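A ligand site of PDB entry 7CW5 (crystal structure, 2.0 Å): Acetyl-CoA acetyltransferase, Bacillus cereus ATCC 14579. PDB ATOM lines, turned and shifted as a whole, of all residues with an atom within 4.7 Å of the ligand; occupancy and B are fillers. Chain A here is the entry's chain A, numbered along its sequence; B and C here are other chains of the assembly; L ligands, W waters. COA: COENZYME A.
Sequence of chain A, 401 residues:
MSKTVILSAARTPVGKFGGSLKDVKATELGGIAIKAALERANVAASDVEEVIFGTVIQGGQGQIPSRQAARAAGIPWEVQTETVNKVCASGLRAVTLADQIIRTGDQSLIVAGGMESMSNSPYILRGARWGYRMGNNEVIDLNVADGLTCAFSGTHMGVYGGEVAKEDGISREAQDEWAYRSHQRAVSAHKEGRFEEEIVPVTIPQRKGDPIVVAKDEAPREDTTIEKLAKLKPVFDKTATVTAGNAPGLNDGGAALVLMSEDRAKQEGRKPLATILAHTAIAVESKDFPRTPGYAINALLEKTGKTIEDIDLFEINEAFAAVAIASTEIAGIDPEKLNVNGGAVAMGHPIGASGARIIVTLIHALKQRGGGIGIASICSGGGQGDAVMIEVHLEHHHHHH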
ATOM      1  N   VAL A  87      18.758   8.506 -16.855  1.00  0.00           N
ATOM      2  CA  VAL A  87      19.178   9.812 -16.259  1.00  0.00           C
ATOM      3  C   VAL A  87      20.471  10.258 -16.965  1.00  0.00           C
ATOM      4  O   VAL A  87      20.435  10.306 -18.200  1.00  0.00           O
ATOM      5  CB  VAL A  87      19.309   9.771 -14.717  1.00  0.00           C
ATOM      6  CG1 VAL A  87      19.226  11.154 -14.114  1.00  0.00           C
ATOM      7  CG2 VAL A  87      18.223   8.917 -14.082  1.00  0.00           C
ATOM      8  N   CYS A  88      21.549  10.595 -16.242  1.00  0.00           N
ATOM      9  CA  CYS A  88      22.818  11.108 -16.830  1.00  0.00           C
ATOM     10  C   CYS A  88      23.390  10.115 -17.866  1.00  0.00           C
ATOM     11  O   CYS A  88      24.160  10.534 -18.732  1.00  0.00           O
ATOM     12  CB  CYS A  88      23.831  11.401 -15.712  1.00  0.00           C
ATOM     13  SG  CYS A  88      23.035  12.102 -14.240  1.00  0.00           S
ATOM     14  N   GLY A 147      14.969  15.086 -12.412  1.00  0.00           N
ATOM     15  CA  GLY A 147      16.404  15.042 -12.764  1.00  0.00           C
ATOM     16  C   GLY A 147      17.341  15.146 -11.559  1.00  0.00           C
ATOM     17  O   GLY A 147      18.313  14.385 -11.505  1.00  0.00           O
ATOM     18  N   LEU A 148      17.104  16.088 -10.643  1.00  0.00           N
ATOM     19  CA  LEU A 148      18.153  16.546  -9.687  1.00  0.00           C
ATOM     20  C   LEU A 148      17.928  15.974  -8.291  1.00  0.00           C
ATOM     21  O   LEU A 148      18.766  16.212  -7.410  1.00  0.00           O
ATOM     22  CB  LEU A 148      18.166  18.074  -9.638  1.00  0.00           C
ATOM     23  CG  LEU A 148      18.575  18.749 -10.942  1.00  0.00           C
ATOM     24  CD1 LEU A 148      18.150  20.209 -10.947  1.00  0.00           C
ATOM     25  CD2 LEU A 148      20.068  18.619 -11.146  1.00  0.00           C
ATOM     26  N   HIS A 156      18.837  16.008  -2.924  1.00  0.00           N
ATOM     27  CA  HIS A 156      19.470  16.535  -4.157  1.00  0.00           C
ATOM     28  C   HIS A 156      20.748  15.726  -4.448  1.00  0.00           C
ATOM     29  O   HIS A 156      21.479  15.381  -3.477  1.00  0.00           O
ATOM     30  CB  HIS A 156      19.678  18.039  -4.021  1.00  0.00           C
ATOM     31  CG  HIS A 156      19.906  18.767  -5.300  1.00  0.00           C
ATOM     32  ND1 HIS A 156      21.053  18.609  -6.047  1.00  0.00           N
ATOM     33  CD2 HIS A 156      19.170  19.719  -5.929  1.00  0.00           C
ATOM     34  CE1 HIS A 156      21.017  19.408  -7.090  1.00  0.00           C
ATOM     35  NE2 HIS A 156      19.874  20.106  -7.041  1.00  0.00           N
ATOM     36  N   MET A 157      21.011  15.458  -5.717  1.00  0.00           N
ATOM     37  CA  MET A 157      22.253  14.766  -6.174  1.00  0.00           C
ATOM     38  C   MET A 157      23.479  15.458  -5.581  1.00  0.00           C
ATOM     39  O   MET A 157      24.465  14.754  -5.237  1.00  0.00           O
ATOM     40  CB  MET A 157      22.364  14.804  -7.697  1.00  0.00           C
ATOM     41  CG  MET A 157      21.262  14.087  -8.441  1.00  0.00           C
ATOM     42  SD  MET A 157      21.102  12.356  -8.000  1.00  0.00           S
ATOM     43  CE  MET A 157      19.693  12.346  -6.890  1.00  0.00           C
ATOM     44  N   HIS A 183      38.075  24.244 -16.472  1.00  0.00           N
ATOM     45  CA  HIS A 183      37.856  25.542 -17.167  1.00  0.00           C
ATOM     46  C   HIS A 183      39.042  25.828 -18.096  1.00  0.00           C
ATOM     47  O   HIS A 183      38.767  26.138 -19.272  1.00  0.00           O
ATOM     48  CB  HIS A 183      37.597  26.683 -16.180  1.00  0.00           C
ATOM     49  CG  HIS A 183      36.180  26.747 -15.719  1.00  0.00           C
ATOM     50  ND1 HIS A 183      35.198  27.401 -16.453  1.00  0.00           N
ATOM     51  CD2 HIS A 183      35.567  26.178 -14.665  1.00  0.00           C
ATOM     52  CE1 HIS A 183      34.045  27.281 -15.822  1.00  0.00           C
ATOM     53  NE2 HIS A 183      34.246  26.539 -14.718  1.00  0.00           N
ATOM     54  N   ARG A 221      34.856  29.497 -18.501  1.00  0.00           N
ATOM     55  CA  ARG A 221      35.268  30.855 -18.053  1.00  0.00           C
ATOM     56  C   ARG A 221      36.784  30.977 -18.144  1.00  0.00           C
ATOM     57  O   ARG A 221      37.512  30.312 -17.355  1.00  0.00           O
ATOM     58  CB  ARG A 221      34.825  31.081 -16.604  1.00  0.00           C
ATOM     59  CG  ARG A 221      33.325  31.177 -16.414  1.00  0.00           C
ATOM     60  CD  ARG A 221      33.068  30.852 -14.956  1.00  0.00           C
ATOM     61  NE  ARG A 221      31.662  30.983 -14.603  1.00  0.00           N
ATOM     62  CZ  ARG A 221      31.101  32.012 -13.980  1.00  0.00           C
ATOM     63  NH1 ARG A 221      29.808  31.987 -13.716  1.00  0.00           N
ATOM     64  NH2 ARG A 221      31.828  33.052 -13.597  1.00  0.00           N
ATOM     65  N   THR A 224      38.109  32.456 -14.694  1.00  0.00           N
ATOM     66  CA  THR A 224      37.925  31.831 -13.352  1.00  0.00           C
ATOM     67  C   THR A 224      39.313  31.541 -12.793  1.00  0.00           C
ATOM     68  O   THR A 224      40.230  31.284 -13.583  1.00  0.00           O
ATOM     69  CB  THR A 224      36.980  30.625 -13.326  1.00  0.00           C
ATOM     70  OG1 THR A 224      36.634  30.428 -11.958  1.00  0.00           O
ATOM     71  CG2 THR A 224      37.600  29.366 -13.884  1.00  0.00           C
ATOM     72  N   LYS A 228      38.827  32.942  -6.812  1.00  0.00           N
ATOM     73  CA  LYS A 228      37.367  33.176  -7.010  1.00  0.00           C
ATOM     74  C   LYS A 228      36.596  31.936  -6.555  1.00  0.00           C
ATOM     75  O   LYS A 228      35.595  32.097  -5.886  1.00  0.00           O
ATOM     76  CB  LYS A 228      37.058  33.543  -8.455  1.00  0.00           C
ATOM     77  CG  LYS A 228      37.625  34.879  -8.899  1.00  0.00           C
ATOM     78  CD  LYS A 228      37.143  35.308 -10.252  1.00  0.00           C
ATOM     79  CE  LYS A 228      38.155  36.176 -10.949  1.00  0.00           C
ATOM     80  NZ  LYS A 228      37.649  36.624 -12.263  1.00  0.00           N
ATOM     81  N   LEU A 229      37.098  30.750  -6.899  1.00  0.00           N
ATOM     82  CA  LEU A 229      36.420  29.476  -6.557  1.00  0.00           C
ATOM     83  C   LEU A 229      36.382  29.282  -5.032  1.00  0.00           C
ATOM     84  O   LEU A 229      35.317  28.874  -4.523  1.00  0.00           O
ATOM     85  CB  LEU A 229      37.176  28.351  -7.280  1.00  0.00           C
ATOM     86  CG  LEU A 229      36.822  28.227  -8.766  1.00  0.00           C
ATOM     87  CD1 LEU A 229      37.866  27.416  -9.506  1.00  0.00           C
ATOM     88  CD2 LEU A 229      35.433  27.616  -8.924  1.00  0.00           C
ATOM     89  N   LEU A 232      33.487  31.004  -3.148  1.00  0.00           N
ATOM     90  CA  LEU A 232      32.071  30.546  -3.298  1.00  0.00           C
ATOM     91  C   LEU A 232      31.598  29.752  -2.072  1.00  0.00           C
ATOM     92  O   LEU A 232      32.403  29.116  -1.389  1.00  0.00           O
ATOM     93  CB  LEU A 232      31.937  29.678  -4.554  1.00  0.00           C
ATOM     94  CG  LEU A 232      32.287  30.404  -5.852  1.00  0.00           C
ATOM     95  CD1 LEU A 232      32.122  29.482  -7.054  1.00  0.00           C
ATOM     96  CD2 LEU A 232      31.449  31.661  -6.015  1.00  0.00           C
ATOM     97  N   VAL A 235      26.638  25.001  -1.633  1.00  0.00           N
ATOM     98  CA  VAL A 235      25.312  25.306  -2.234  1.00  0.00           C
ATOM     99  C   VAL A 235      24.219  24.432  -1.586  1.00  0.00           C
ATOM    100  O   VAL A 235      23.141  24.993  -1.298  1.00  0.00           O
ATOM    101  CB  VAL A 235      25.353  25.230  -3.775  1.00  0.00           C
ATOM    102  CG1 VAL A 235      25.307  23.819  -4.302  1.00  0.00           C
ATOM    103  CG2 VAL A 235      24.255  26.055  -4.405  1.00  0.00           C
ATOM    104  N   PHE A 236      24.473  23.169  -1.249  1.00  0.00           N
ATOM    105  CA  PHE A 236      23.439  22.180  -0.815  1.00  0.00           C
ATOM    106  C   PHE A 236      23.467  21.961   0.705  1.00  0.00           C
ATOM    107  O   PHE A 236      22.457  21.473   1.240  1.00  0.00           O
ATOM    108  CB  PHE A 236      23.629  20.840  -1.524  1.00  0.00           C
ATOM    109  CG  PHE A 236      23.708  20.972  -3.025  1.00  0.00           C
ATOM    110  CD1 PHE A 236      22.558  21.202  -3.769  1.00  0.00           C
ATOM    111  CD2 PHE A 236      24.922  20.896  -3.690  1.00  0.00           C
ATOM    112  CE1 PHE A 236      22.619  21.341  -5.144  1.00  0.00           C
ATOM    113  CE2 PHE A 236      24.980  21.014  -5.078  1.00  0.00           C
ATOM    114  CZ  PHE A 236      23.827  21.244  -5.797  1.00  0.00           C
ATOM    115  N   ALA A 244      28.732  26.010  -6.596  1.00  0.00           N
ATOM    116  CA  ALA A 244      28.356  26.297  -7.996  1.00  0.00           C
ATOM    117  C   ALA A 244      29.584  26.221  -8.910  1.00  0.00           C
ATOM    118  O   ALA A 244      29.376  26.093 -10.142  1.00  0.00           O
ATOM    119  CB  ALA A 244      27.731  27.672  -8.069  1.00  0.00           C
ATOM    120  N   GLY A 245      30.790  26.401  -8.364  1.00  0.00           N
ATOM    121  CA  GLY A 245      32.042  26.518  -9.141  1.00  0.00           C
ATOM    122  C   GLY A 245      32.724  25.186  -9.390  1.00  0.00           C
ATOM    123  O   GLY A 245      33.454  25.072 -10.387  1.00  0.00           O
ATOM    124  N   ALA A 247      30.792  22.215  -9.174  1.00  0.00           N
ATOM    125  CA  ALA A 247      29.731  21.338  -9.682  1.00  0.00           C
ATOM    126  C   ALA A 247      29.301  21.878 -11.031  1.00  0.00           C
ATOM    127  O   ALA A 247      29.238  23.092 -11.205  1.00  0.00           O
ATOM    128  CB  ALA A 247      28.560  21.275  -8.743  1.00  0.00           C
ATOM    129  N   PRO A 248      28.924  20.985 -11.977  1.00  0.00           N
ATOM    130  CA  PRO A 248      28.407  21.421 -13.276  1.00  0.00           C
ATOM    131  C   PRO A 248      27.079  22.144 -13.066  1.00  0.00           C
ATOM    132  O   PRO A 248      26.485  21.980 -11.996  1.00  0.00           O
ATOM    133  CB  PRO A 248      28.230  20.119 -14.059  1.00  0.00           C
ATOM    134  CG  PRO A 248      27.983  19.092 -12.996  1.00  0.00           C
ATOM    135  CD  PRO A 248      28.845  19.523 -11.819  1.00  0.00           C
ATOM    136  N   GLY A 249      26.666  22.914 -14.074  1.00  0.00           N
ATOM    137  CA  GLY A 249      25.378  23.623 -14.106  1.00  0.00           C
ATOM    138  C   GLY A 249      24.238  22.729 -14.586  1.00  0.00           C
ATOM    139  O   GLY A 249      24.419  21.505 -14.707  1.00  0.00           O
ATOM    140  N   LEU A 250      23.095  23.379 -14.775  1.00  0.00           N
ATOM    141  CA  LEU A 250      21.926  22.952 -15.592  1.00  0.00           C
ATOM    142  C   LEU A 250      22.197  23.491 -16.996  1.00  0.00           C
ATOM    143  O   LEU A 250      22.658  24.634 -17.084  1.00  0.00           O
ATOM    144  CB  LEU A 250      20.661  23.585 -15.007  1.00  0.00           C
ATOM    145  CG  LEU A 250      20.052  22.885 -13.795  1.00  0.00           C
ATOM    146  CD1 LEU A 250      21.072  22.681 -12.724  1.00  0.00           C
ATOM    147  CD2 LEU A 250      18.851  23.657 -13.254  1.00  0.00           C
ATOM    148  N   PHE A 320      30.423  15.898 -10.398  1.00  0.00           N
ATOM    149  CA  PHE A 320      31.077  16.906  -9.522  1.00  0.00           C
ATOM    150  C   PHE A 320      32.571  16.844  -9.794  1.00  0.00           C
ATOM    151  O   PHE A 320      33.006  15.807 -10.329  1.00  0.00           O
ATOM    152  CB  PHE A 320      30.738  16.580  -8.077  1.00  0.00           C
ATOM    153  CG  PHE A 320      29.251  16.539  -7.839  1.00  0.00           C
ATOM    154  CD1 PHE A 320      28.539  17.699  -7.674  1.00  0.00           C
ATOM    155  CD2 PHE A 320      28.581  15.338  -7.856  1.00  0.00           C
ATOM    156  CE1 PHE A 320      27.168  17.668  -7.484  1.00  0.00           C
ATOM    157  CE2 PHE A 320      27.204  15.292  -7.643  1.00  0.00           C
ATOM    158  CZ  PHE A 320      26.500  16.458  -7.481  1.00  0.00           C
ATOM    159  N   HIS A 349      26.428  20.154 -17.957  1.00  0.00           N
ATOM    160  CA  HIS A 349      25.846  18.801 -17.865  1.00  0.00           C
ATOM    161  C   HIS A 349      24.393  18.834 -18.332  1.00  0.00           C
ATOM    162  O   HIS A 349      23.493  18.874 -17.498  1.00  0.00           O
ATOM    163  CB  HIS A 349      26.009  18.282 -16.437  1.00  0.00           C
ATOM    164  CG  HIS A 349      25.497  16.899 -16.227  1.00  0.00           C
ATOM    165  ND1 HIS A 349      25.390  15.971 -17.267  1.00  0.00           N
ATOM    166  CD2 HIS A 349      25.095  16.267 -15.114  1.00  0.00           C
ATOM    167  CE1 HIS A 349      24.931  14.839 -16.776  1.00  0.00           C
ATOM    168  NE2 HIS A 349      24.763  14.986 -15.453  1.00  0.00           N
ATOM    169  N   ILE A 351      21.714  16.883 -19.095  1.00  0.00           N
ATOM    170  CA  ILE A 351      21.683  15.516 -18.532  1.00  0.00           C
ATOM    171  C   ILE A 351      21.565  14.469 -19.644  1.00  0.00           C
ATOM    172  O   ILE A 351      22.423  13.566 -19.703  1.00  0.00           O
ATOM    173  CB  ILE A 351      20.538  15.355 -17.510  1.00  0.00           C
ATOM    174  CG1 ILE A 351      20.648  16.350 -16.345  1.00  0.00           C
ATOM    175  CG2 ILE A 351      20.535  13.931 -17.006  1.00  0.00           C
ATOM    176  CD1 ILE A 351      19.517  16.208 -15.350  1.00  0.00           C
ATOM    177  N   GLY A 381      22.122   9.601 -11.799  1.00  0.00           N
ATOM    178  CA  GLY A 381      21.249   9.677 -10.616  1.00  0.00           C
ATOM    179  C   GLY A 381      20.480   8.400 -10.502  1.00  0.00           C
ATOM    180  O   GLY A 381      20.168   7.831 -11.551  1.00  0.00           O
ATOM    181  N   ARG B 133      12.390  30.822 -12.373  1.00  0.00           N
ATOM    182  CA  ARG B 133      13.797  30.539 -12.765  1.00  0.00           C
ATOM    183  C   ARG B 133      14.156  29.095 -12.390  1.00  0.00           C
ATOM    184  O   ARG B 133      14.321  28.289 -13.312  1.00  0.00           O
ATOM    185  CB  ARG B 133      14.774  31.541 -12.121  1.00  0.00           C
ATOM    186  CG  ARG B 133      16.227  31.176 -12.415  1.00  0.00           C
ATOM    187  CD  ARG B 133      17.276  32.225 -12.111  1.00  0.00           C
ATOM    188  NE  ARG B 133      18.557  31.911 -12.739  1.00  0.00           N
ATOM    189  CZ  ARG B 133      19.554  31.224 -12.180  1.00  0.00           C
ATOM    190  NH1 ARG B 133      19.442  30.762 -10.950  1.00  0.00           N
ATOM    191  NH2 ARG B 133      20.667  31.006 -12.862  1.00  0.00           N
ATOM    192  N   MET B 134      14.275  28.761 -11.101  1.00  0.00           N
ATOM    193  CA  MET B 134      14.488  27.359 -10.663  1.00  0.00           C
ATOM    194  C   MET B 134      14.060  27.186  -9.201  1.00  0.00           C
ATOM    195  O   MET B 134      13.990  28.152  -8.496  1.00  0.00           O
ATOM    196  CB  MET B 134      15.957  26.897 -10.833  1.00  0.00           C
ATOM    197  CG  MET B 134      16.951  27.577  -9.945  1.00  0.00           C
ATOM    198  SD  MET B 134      18.591  26.815 -10.088  1.00  0.00           S
ATOM    199  CE  MET B 134      19.100  27.296 -11.734  1.00  0.00           C
ATOM    200  N   GLN C  63      13.014  10.457 -10.885  1.00  0.00           N
ATOM    201  CA  GLN C  63      14.207   9.867 -11.539  1.00  0.00           C
ATOM    202  C   GLN C  63      13.934   8.423 -11.985  1.00  0.00           C
ATOM    203  O   GLN C  63      13.463   7.616 -11.153  1.00  0.00           O
ATOM    204  CB  GLN C  63      15.389   9.846 -10.580  1.00  0.00           C
ATOM    205  CG  GLN C  63      16.316  11.033 -10.715  1.00  0.00           C
ATOM    206  CD  GLN C  63      17.532  10.840  -9.873  1.00  0.00           C
ATOM    207  OE1 GLN C  63      17.590   9.921  -9.047  1.00  0.00           O
ATOM    208  NE2 GLN C  63      18.484  11.744 -10.026  1.00  0.00           N
HETATM  209  N1A COA L   1      34.165  30.953 -11.252  1.00  0.00           N
HETATM  210  C2A COA L   1      33.636  32.042 -10.669  1.00  0.00           C
HETATM  211  N3A COA L   1      32.392  32.261 -10.273  1.00  0.00           N
HETATM  212  C4A COA L   1      31.610  31.185 -10.506  1.00  0.00           C
HETATM  213  C5A COA L   1      32.000  30.001 -11.089  1.00  0.00           C
HETATM  214  C6A COA L   1      33.338  29.889 -11.482  1.00  0.00           C
HETATM  215  N6A COA L   1      33.842  28.799 -12.063  1.00  0.00           N
HETATM  216  N7A COA L   1      30.914  29.127 -11.181  1.00  0.00           N
HETATM  217  C8A COA L   1      29.915  29.790 -10.652  1.00  0.00           C
HETATM  218  N9A COA L   1      30.278  31.038 -10.232  1.00  0.00           N
HETATM  219  C1B COA L   1      29.418  32.035  -9.638  1.00  0.00           C
HETATM  220  C2B COA L   1      28.385  32.567 -10.643  1.00  0.00           C
HETATM  221  O2B COA L   1      28.870  33.686 -11.345  1.00  0.00           O
HETATM  222  C3B COA L   1      27.197  32.852  -9.714  1.00  0.00           C
HETATM  223  O3B COA L   1      27.406  34.114  -9.047  1.00  0.00           O
HETATM  224  P3B COA L   1      26.392  35.332  -9.457  1.00  0.00           P
HETATM  225  O7A COA L   1      27.055  36.601  -8.930  1.00  0.00           O
HETATM  226  O8A COA L   1      25.009  35.072  -8.808  1.00  0.00           O
HETATM  227  O9A COA L   1      26.317  35.315 -10.993  1.00  0.00           O
HETATM  228  C4B COA L   1      27.293  31.689  -8.710  1.00  0.00           C
HETATM  229  O4B COA L   1      28.708  31.411  -8.600  1.00  0.00           O
HETATM  230  C5B COA L   1      26.629  30.384  -9.082  1.00  0.00           C
HETATM  231  O5B COA L   1      25.380  30.621  -9.737  1.00  0.00           O
HETATM  232  P1A COA L   1      24.920  29.928 -11.108  1.00  0.00           P
HETATM  233  O1A COA L   1      26.076  29.606 -11.993  1.00  0.00           O
HETATM  234  O2A COA L   1      23.833  30.770 -11.684  1.00  0.00           O
HETATM  235  O3A COA L   1      24.271  28.573 -10.555  1.00  0.00           O
HETATM  236  P2A COA L   1      22.791  28.383  -9.957  1.00  0.00           P
HETATM  237  O4A COA L   1      22.719  29.045  -8.616  1.00  0.00           O
HETATM  238  O5A COA L   1      21.784  28.772 -10.990  1.00  0.00           O
HETATM  239  O6A COA L   1      22.786  26.806  -9.755  1.00  0.00           O
HETATM  240  CBP COA L   1      23.661  24.749  -8.893  1.00  0.00           C
HETATM  241  CCP COA L   1      23.999  26.183  -9.253  1.00  0.00           C
HETATM  242  CDP COA L   1      24.931  24.102  -8.323  1.00  0.00           C
HETATM  243  CEP COA L   1      22.530  24.751  -7.838  1.00  0.00           C
HETATM  244  CAP COA L   1      23.182  23.990 -10.140  1.00  0.00           C
HETATM  245  OAP COA L   1      24.053  24.239 -11.240  1.00  0.00           O
HETATM  246  C9P COA L   1      23.093  22.513  -9.909  1.00  0.00           C
HETATM  247  O9P COA L   1      22.184  22.071  -9.202  1.00  0.00           O
HETATM  248  N8P COA L   1      24.046  21.760 -10.452  1.00  0.00           N
HETATM  249  C7P COA L   1      24.093  20.311 -10.312  1.00  0.00           C
HETATM  250  C6P COA L   1      23.488  19.618 -11.502  1.00  0.00           C
HETATM  251  C5P COA L   1      23.449  18.117 -11.349  1.00  0.00           C
HETATM  252  O5P COA L   1      23.651  17.587 -10.254  1.00  0.00           O
HETATM  253  N4P COA L   1      23.153  17.407 -12.443  1.00  0.00           N
HETATM  254  C3P COA L   1      22.982  15.961 -12.451  1.00  0.00           C
HETATM  255  C2P COA L   1      21.606  15.523 -11.964  1.00  0.00           C
HETATM  256  S1P COA L   1      21.318  13.739 -12.084  1.00  0.00           S
HETATM  257  O   HOH W   1      32.517  26.052 -12.501  1.00  0.00           O
HETATM  258  O   HOH W   2      27.079  24.935 -10.876  1.00  0.00           O
HETATM  259  O   HOH W   3      32.029  34.447  -8.686  1.00  0.00           O
HETATM  260  O   HOH W   4      23.137  25.904 -13.632  1.00  0.00           O
HETATM  261  O   HOH W   5      25.513  15.441 -11.293  1.00  0.00           O
HETATM  262  O   HOH W   6      29.429  34.832  -6.465  1.00  0.00           O
HETATM  263  O   HOH W   7      19.728  22.431  -8.625  1.00  0.00           O
HETATM  264  O   HOH W   8      28.092  29.686 -13.737  1.00  0.00           O
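A sulfur (S1P) of the ligand sits close to the side-chain sulfur of Cys 88, 3.2 Å away.
The backbone carbonyl oxygen of Pro 248 lies within hydrogen-bond range of a nitrogen (N8P) of the ligand (2.9 Å).
O5A of the ligand is in salt-bridge range of NH1 of Arg 133 of chain B (3.1 Å).
O of Gly 147 sits close to S1P of the ligand, at 3.1 Å.
An oxygen (O2B) of the ligand lies within hydrogen-bond range of the guanidinium group (NH1) of Arg 221.
A nitrogen (N1A) of the ligand sits at hydrogen-bond distance from the side-chain hydroxyl (OG1) of Thr 224, at 2.6 Å.
A ring nitrogen (ND1) of His 183 is in hydrogen-bond range of the backbone NH of Arg 221, 3.0 Å away.
The side-chain sulfur (SG) of Cys 88 sits at hydrogen-bond distance from a ring nitrogen (NE2) of His 349 (3.6 Å).
The side-chain sulfur of Cys 88 lies within hydrogen-bond range of the backbone NH of Gly 381.
The backbone carbonyl oxygen of Gly 147 sits at hydrogen-bond distance from the side-chain amide nitrogen of Gln 63 of chain C (3.0 Å).
The side-chain sulfur (SD) of Met 157 sits at hydrogen-bond distance from the side-chain amide nitrogen (NE2) of Gln 63 of chain C (3.4 Å).
The backbone carbonyl oxygen (O) of Leu 148 is in hydrogen-bond range of the backbone NH (N) of Met 157 (2.9 Å).
Residues that only touch the ligand: Val 87, Leu 148, His 156, Met 157, His 183, Leu 229, Leu 232, Phe 236, Ala 244, Gly 245, Gly 249, Leu 250, His 349 and Met 134 of chain B.
Hydrophobic or aromatic side chains within 4 Å of the ligand: Val 87, Leu 148, His 156, Met 157, Leu 229, Leu 232, Phe 236, Ala 244, Leu 250, His 349 and Met 134 of chain B.
The nearest printed residue that does not touch the ligand is Gln 63 of chain C (4.03 Å).
Water W7 bridges an oxygen (O9P) of the ligand (2.5 Å) and a ring nitrogen (NE2) of His 156 (2.8 Å).
Water W8 bridges O1A of the ligand (2.7 Å) and NH1 of Arg 221 (2.9 Å).
Water W4 bridges the backbone NH (N) of Leu 250 (2.8 Å) and an oxygen (OAP) of the ligand (3.1 Å).
Water W1 lies within hydrogen-bond range of the backbone carbonyl oxygen (O) of Gly 245, a ring nitrogen (NE2) of His 183 and a nitrogen (N6A) of the ligand.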
